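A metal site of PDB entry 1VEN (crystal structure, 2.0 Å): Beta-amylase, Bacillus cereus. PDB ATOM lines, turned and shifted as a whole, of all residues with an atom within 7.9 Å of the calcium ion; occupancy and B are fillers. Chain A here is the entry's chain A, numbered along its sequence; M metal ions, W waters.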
ATOM      1  N   TRP A  52      13.805  15.672  18.244  1.00  0.00           N
ATOM      2  CA  TRP A  52      13.562  14.894  19.440  1.00  0.00           C
ATOM      3  C   TRP A  52      12.105  15.140  19.858  1.00  0.00           C
ATOM      4  O   TRP A  52      11.418  14.232  20.322  1.00  0.00           O
ATOM      5  CB  TRP A  52      14.532  15.329  20.538  1.00  0.00           C
ATOM      6  CG  TRP A  52      14.469  14.495  21.797  1.00  0.00           C
ATOM      7  CD1 TRP A  52      13.939  13.246  21.934  1.00  0.00           C
ATOM      8  CD2 TRP A  52      14.987  14.851  23.083  1.00  0.00           C
ATOM      9  NE1 TRP A  52      14.095  12.802  23.224  1.00  0.00           N
ATOM     10  CE2 TRP A  52      14.733  13.769  23.957  1.00  0.00           C
ATOM     11  CE3 TRP A  52      15.652  15.979  23.582  1.00  0.00           C
ATOM     12  CZ2 TRP A  52      15.120  13.782  25.297  1.00  0.00           C
ATOM     13  CZ3 TRP A  52      16.030  16.002  24.918  1.00  0.00           C
ATOM     14  CH2 TRP A  52      15.764  14.901  25.768  1.00  0.00           C
ATOM     15  N   GLU A  56      10.024  11.416  20.554  1.00  0.00           N
ATOM     16  CA  GLU A  56       9.754  10.956  21.912  1.00  0.00           C
ATOM     17  C   GLU A  56       8.856  11.988  22.591  1.00  0.00           C
ATOM     18  O   GLU A  56       9.100  12.407  23.727  1.00  0.00           O
ATOM     19  CB  GLU A  56      11.081  10.786  22.662  1.00  0.00           C
ATOM     20  CG  GLU A  56      10.978  10.145  24.036  1.00  0.00           C
ATOM     21  CD  GLU A  56      12.351   9.900  24.668  1.00  0.00           C
ATOM     22  OE1 GLU A  56      13.311  10.583  24.275  1.00  0.00           O
ATOM     23  OE2 GLU A  56      12.461   9.030  25.567  1.00  0.00           O
ATOM     24  N   GLY A  59       6.012  10.727  25.978  1.00  0.00           N
ATOM     25  CA  GLY A  59       6.640  10.534  27.260  1.00  0.00           C
ATOM     26  C   GLY A  59       7.923   9.746  27.142  1.00  0.00           C
ATOM     27  O   GLY A  59       8.290   9.294  26.054  1.00  0.00           O
ATOM     28  N   ASP A  60       8.597   9.576  28.264  1.00  0.00           N
ATOM     29  CA  ASP A  60       9.847   8.830  28.301  1.00  0.00           C
ATOM     30  C   ASP A  60       9.662   7.424  27.717  1.00  0.00           C
ATOM     31  O   ASP A  60       8.782   6.670  28.125  1.00  0.00           O
ATOM     32  CB  ASP A  60      10.361   8.756  29.739  1.00  0.00           C
ATOM     33  CG  ASP A  60      11.729   8.137  29.828  1.00  0.00           C
ATOM     34  OD1 ASP A  60      12.552   8.335  28.915  1.00  0.00           O
ATOM     35  OD2 ASP A  60      12.007   7.459  30.844  1.00  0.00           O
ATOM     36  N   GLN A  61      10.504   7.106  26.736  1.00  0.00           N
ATOM     37  CA  GLN A  61      10.489   5.804  26.061  1.00  0.00           C
ATOM     38  C   GLN A  61       9.270   5.533  25.176  1.00  0.00           C
ATOM     39  O   GLN A  61       9.043   4.390  24.768  1.00  0.00           O
ATOM     40  CB  GLN A  61      10.658   4.668  27.087  1.00  0.00           C
ATOM     41  CG  GLN A  61      11.962   4.723  27.898  1.00  0.00           C
ATOM     42  CD  GLN A  61      13.199   4.977  27.043  1.00  0.00           C
ATOM     43  OE1 GLN A  61      13.541   6.124  26.744  1.00  0.00           O
ATOM     44  NE2 GLN A  61      13.875   3.909  26.644  1.00  0.00           N
ATOM     45  N   GLN A  62       8.479   6.568  24.915  1.00  0.00           N
ATOM     46  CA  GLN A  62       7.319   6.440  24.025  1.00  0.00           C
ATOM     47  C   GLN A  62       7.780   7.019  22.694  1.00  0.00           C
ATOM     48  O   GLN A  62       7.527   8.191  22.387  1.00  0.00           O
ATOM     49  CB  GLN A  62       6.124   7.234  24.567  1.00  0.00           C
ATOM     50  CG  GLN A  62       5.293   6.470  25.588  1.00  0.00           C
ATOM     51  CD  GLN A  62       4.112   7.266  26.081  1.00  0.00           C
ATOM     52  OE1 GLN A  62       4.248   8.154  26.931  1.00  0.00           O
ATOM     53  NE2 GLN A  62       2.926   6.983  25.539  1.00  0.00           N
ATOM     54  N   PHE A  63       8.465   6.185  21.919  1.00  0.00           N
ATOM     55  CA  PHE A  63       9.037   6.581  20.644  1.00  0.00           C
ATOM     56  C   PHE A  63       8.126   6.492  19.426  1.00  0.00           C
ATOM     57  O   PHE A  63       7.149   5.748  19.398  1.00  0.00           O
ATOM     58  CB  PHE A  63      10.294   5.766  20.363  1.00  0.00           C
ATOM     59  CG  PHE A  63      11.408   5.976  21.363  1.00  0.00           C
ATOM     60  CD1 PHE A  63      12.003   7.228  21.515  1.00  0.00           C
ATOM     61  CD2 PHE A  63      11.893   4.912  22.125  1.00  0.00           C
ATOM     62  CE1 PHE A  63      13.069   7.419  22.422  1.00  0.00           C
ATOM     63  CE2 PHE A  63      12.953   5.086  23.019  1.00  0.00           C
ATOM     64  CZ  PHE A  63      13.548   6.343  23.163  1.00  0.00           C
ATOM     65  N   TRP A 106       8.025  16.799  28.875  1.00  0.00           N
ATOM     66  CA  TRP A 106       8.165  15.986  30.080  1.00  0.00           C
ATOM     67  C   TRP A 106       9.600  15.907  30.612  1.00  0.00           C
ATOM     68  O   TRP A 106       9.811  15.628  31.791  1.00  0.00           O
ATOM     69  CB  TRP A 106       7.649  14.565  29.837  1.00  0.00           C
ATOM     70  CG  TRP A 106       8.288  13.892  28.666  1.00  0.00           C
ATOM     71  CD1 TRP A 106       7.764  13.791  27.413  1.00  0.00           C
ATOM     72  CD2 TRP A 106       9.554  13.231  28.638  1.00  0.00           C
ATOM     73  NE1 TRP A 106       8.629  13.098  26.595  1.00  0.00           N
ATOM     74  CE2 TRP A 106       9.744  12.754  27.319  1.00  0.00           C
ATOM     75  CE3 TRP A 106      10.562  13.012  29.594  1.00  0.00           C
ATOM     76  CZ2 TRP A 106      10.892  12.058  26.936  1.00  0.00           C
ATOM     77  CZ3 TRP A 106      11.709  12.317  29.211  1.00  0.00           C
ATOM     78  CH2 TRP A 106      11.862  11.847  27.889  1.00  0.00           C
ATOM     79  N   VAL A 107      10.581  16.150  29.751  1.00  0.00           N
ATOM     80  CA  VAL A 107      11.970  16.087  30.178  1.00  0.00           C
ATOM     81  C   VAL A 107      12.239  17.115  31.284  1.00  0.00           C
ATOM     82  O   VAL A 107      13.060  16.895  32.161  1.00  0.00           O
ATOM     83  CB  VAL A 107      12.941  16.334  29.003  1.00  0.00           C
ATOM     84  CG1 VAL A 107      12.988  17.814  28.661  1.00  0.00           C
ATOM     85  CG2 VAL A 107      14.325  15.828  29.353  1.00  0.00           C
ATOM     86  N   GLN A 110      11.933  16.110  35.143  1.00  0.00           N
ATOM     87  CA  GLN A 110      12.795  15.097  35.730  1.00  0.00           C
ATOM     88  C   GLN A 110      13.778  15.645  36.771  1.00  0.00           C
ATOM     89  O   GLN A 110      14.563  14.883  37.334  1.00  0.00           O
ATOM     90  CB  GLN A 110      13.546  14.335  34.632  1.00  0.00           C
ATOM     91  CG  GLN A 110      12.671  13.331  33.910  1.00  0.00           C
ATOM     92  CD  GLN A 110      13.467  12.209  33.265  1.00  0.00           C
ATOM     93  OE1 GLN A 110      12.911  11.178  32.883  1.00  0.00           O
ATOM     94  NE2 GLN A 110      14.772  12.414  33.128  1.00  0.00           N
ATOM     95  N   VAL A 137      21.251  13.424  33.197  1.00  0.00           N
ATOM     96  CA  VAL A 137      20.024  13.374  32.406  1.00  0.00           C
ATOM     97  C   VAL A 137      20.370  13.163  30.926  1.00  0.00           C
ATOM     98  O   VAL A 137      19.730  12.371  30.230  1.00  0.00           O
ATOM     99  CB  VAL A 137      19.208  14.674  32.540  1.00  0.00           C
ATOM    100  CG1 VAL A 137      18.050  14.679  31.549  1.00  0.00           C
ATOM    101  CG2 VAL A 137      18.693  14.815  33.977  1.00  0.00           C
ATOM    102  N   LYS A 140      21.280   9.615  30.204  1.00  0.00           N
ATOM    103  CA  LYS A 140      20.103   8.763  30.169  1.00  0.00           C
ATOM    104  C   LYS A 140      19.276   8.947  28.889  1.00  0.00           C
ATOM    105  O   LYS A 140      19.051   7.983  28.153  1.00  0.00           O
ATOM    106  CB  LYS A 140      19.197   9.037  31.371  1.00  0.00           C
ATOM    107  CG  LYS A 140      17.900   8.233  31.346  1.00  0.00           C
ATOM    108  CD  LYS A 140      16.945   8.606  32.463  1.00  0.00           C
ATOM    109  CE  LYS A 140      15.647   7.801  32.388  1.00  0.00           C
ATOM    110  NZ  LYS A 140      14.853   8.118  31.160  1.00  0.00           N
ATOM    111  N   GLU A 141      18.824  10.167  28.637  1.00  0.00           N
ATOM    112  CA  GLU A 141      17.979  10.436  27.467  1.00  0.00           C
ATOM    113  C   GLU A 141      18.661  10.277  26.098  1.00  0.00           C
ATOM    114  O   GLU A 141      18.130   9.616  25.213  1.00  0.00           O
ATOM    115  CB  GLU A 141      17.370  11.834  27.587  1.00  0.00           C
ATOM    116  CG  GLU A 141      16.583  12.084  28.870  1.00  0.00           C
ATOM    117  CD  GLU A 141      15.586  10.976  29.202  1.00  0.00           C
ATOM    118  OE1 GLU A 141      15.001  10.395  28.268  1.00  0.00           O
ATOM    119  OE2 GLU A 141      15.375  10.704  30.404  1.00  0.00           O
ATOM    120  N   TYR A 142      19.824  10.906  25.905  1.00  0.00           N
ATOM    121  CA  TYR A 142      20.500  10.792  24.618  1.00  0.00           C
ATOM    122  C   TYR A 142      20.859   9.337  24.410  1.00  0.00           C
ATOM    123  O   TYR A 142      20.743   8.813  23.297  1.00  0.00           O
ATOM    124  CB  TYR A 142      21.760  11.656  24.579  1.00  0.00           C
ATOM    125  CG  TYR A 142      21.513  13.154  24.439  1.00  0.00           C
ATOM    126  CD1 TYR A 142      20.373  13.758  24.989  1.00  0.00           C
ATOM    127  CD2 TYR A 142      22.452  13.986  23.810  1.00  0.00           C
ATOM    128  CE1 TYR A 142      20.184  15.148  24.914  1.00  0.00           C
ATOM    129  CE2 TYR A 142      22.271  15.371  23.731  1.00  0.00           C
ATOM    130  CZ  TYR A 142      21.135  15.946  24.297  1.00  0.00           C
ATOM    131  OH  TYR A 142      20.985  17.312  24.251  1.00  0.00           O
ATOM    132  N   GLY A 143      21.285   8.679  25.486  1.00  0.00           N
ATOM    133  CA  GLY A 143      21.652   7.278  25.400  1.00  0.00           C
ATOM    134  C   GLY A 143      20.497   6.446  24.876  1.00  0.00           C
ATOM    135  O   GLY A 143      20.663   5.692  23.904  1.00  0.00           O
ATOM    136  N   GLU A 144      19.333   6.592  25.500  1.00  0.00           N
ATOM    137  CA  GLU A 144      18.139   5.853  25.106  1.00  0.00           C
ATOM    138  C   GLU A 144      17.667   6.254  23.709  1.00  0.00           C
ATOM    139  O   GLU A 144      17.265   5.383  22.921  1.00  0.00           O
ATOM    140  CB  GLU A 144      17.016   6.087  26.119  1.00  0.00           C
ATOM    141  CG  GLU A 144      17.383   5.671  27.529  1.00  0.00           C
ATOM    142  CD  GLU A 144      16.339   6.056  28.540  1.00  0.00           C
ATOM    143  OE1 GLU A 144      15.800   7.189  28.444  1.00  0.00           O
ATOM    144  OE2 GLU A 144      16.064   5.244  29.446  1.00  0.00           O
ATOM    145  N   LEU A 145      17.726   7.543  23.391  1.00  0.00           N
ATOM    146  CA  LEU A 145      17.295   8.020  22.079  1.00  0.00           C
ATOM    147  C   LEU A 145      18.141   7.451  20.935  1.00  0.00           C
ATOM    148  O   LEU A 145      17.597   6.928  19.964  1.00  0.00           O
ATOM    149  CB  LEU A 145      17.315   9.555  22.011  1.00  0.00           C
ATOM    150  CG  LEU A 145      16.861  10.145  20.670  1.00  0.00           C
ATOM    151  CD1 LEU A 145      15.432   9.718  20.371  1.00  0.00           C
ATOM    152  CD2 LEU A 145      16.948  11.665  20.719  1.00  0.00           C
HETATM  153 CA    CA M   1      14.073   8.393  27.320  1.00  0.00          CA
HETATM  154  O   HOH W   1      15.492   9.084  25.405  1.00  0.00           O
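Residues that only touch the calcium ion: Lys 140 (3.9 Å). Six residues have an atom within 4 Å of the calcium ion: Glu 56, Asp 60, Gln 61, Lys 140, Glu 141 and Glu 144. Along chain A the residues within 4 Å of the calcium ion span positions 56 to 144.
OE2 of Glu 144 lies within salt-bridge range of NZ of Lys 140. OD2 of Asp 60 is in salt-bridge range of NZ of Lys 140 (2.9 Å). The side-chain carboxylate (OE2) of Glu 141 lies within salt-bridge range of the side-chain amino group (NZ) of Lys 140 (2.7 Å). The backbone carbonyl oxygen of Glu 56 is in hydrogen-bond range of the indole nitrogen of Trp 106 (3.0 Å). NE1 of Trp 52 sits at hydrogen-bond distance from OE1 of Glu 56. The side-chain amide nitrogen of Gln 110 is in hydrogen-bond range of the side-chain carboxylate of Glu 141 (3.3 Å).
The side-chain carboxylate (OD1) of Asp 60 is bound to the calcium ion (2.2 Å). OE1 of Glu 144 binds the calcium ion (2.4 Å). The calcium ion is bound by the side-chain amide oxygen (OE1) of Gln 61 (2.4 Å). OE1 of Glu 141 is bound to the calcium ion, at 2.4 Å. The calcium ion is bound by OE2 of Glu 56 (2.5 Å). The calcium ion is bound by water W1, 2.5 Å away. The calcium ion has six donor atoms within binding distance.
Water W1 lies within hydrogen-bond range of O of Glu 141 (2.7 Å), OE1 of Glu 56 (2.9 Å) and N of Leu 145 (3.4 Å).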
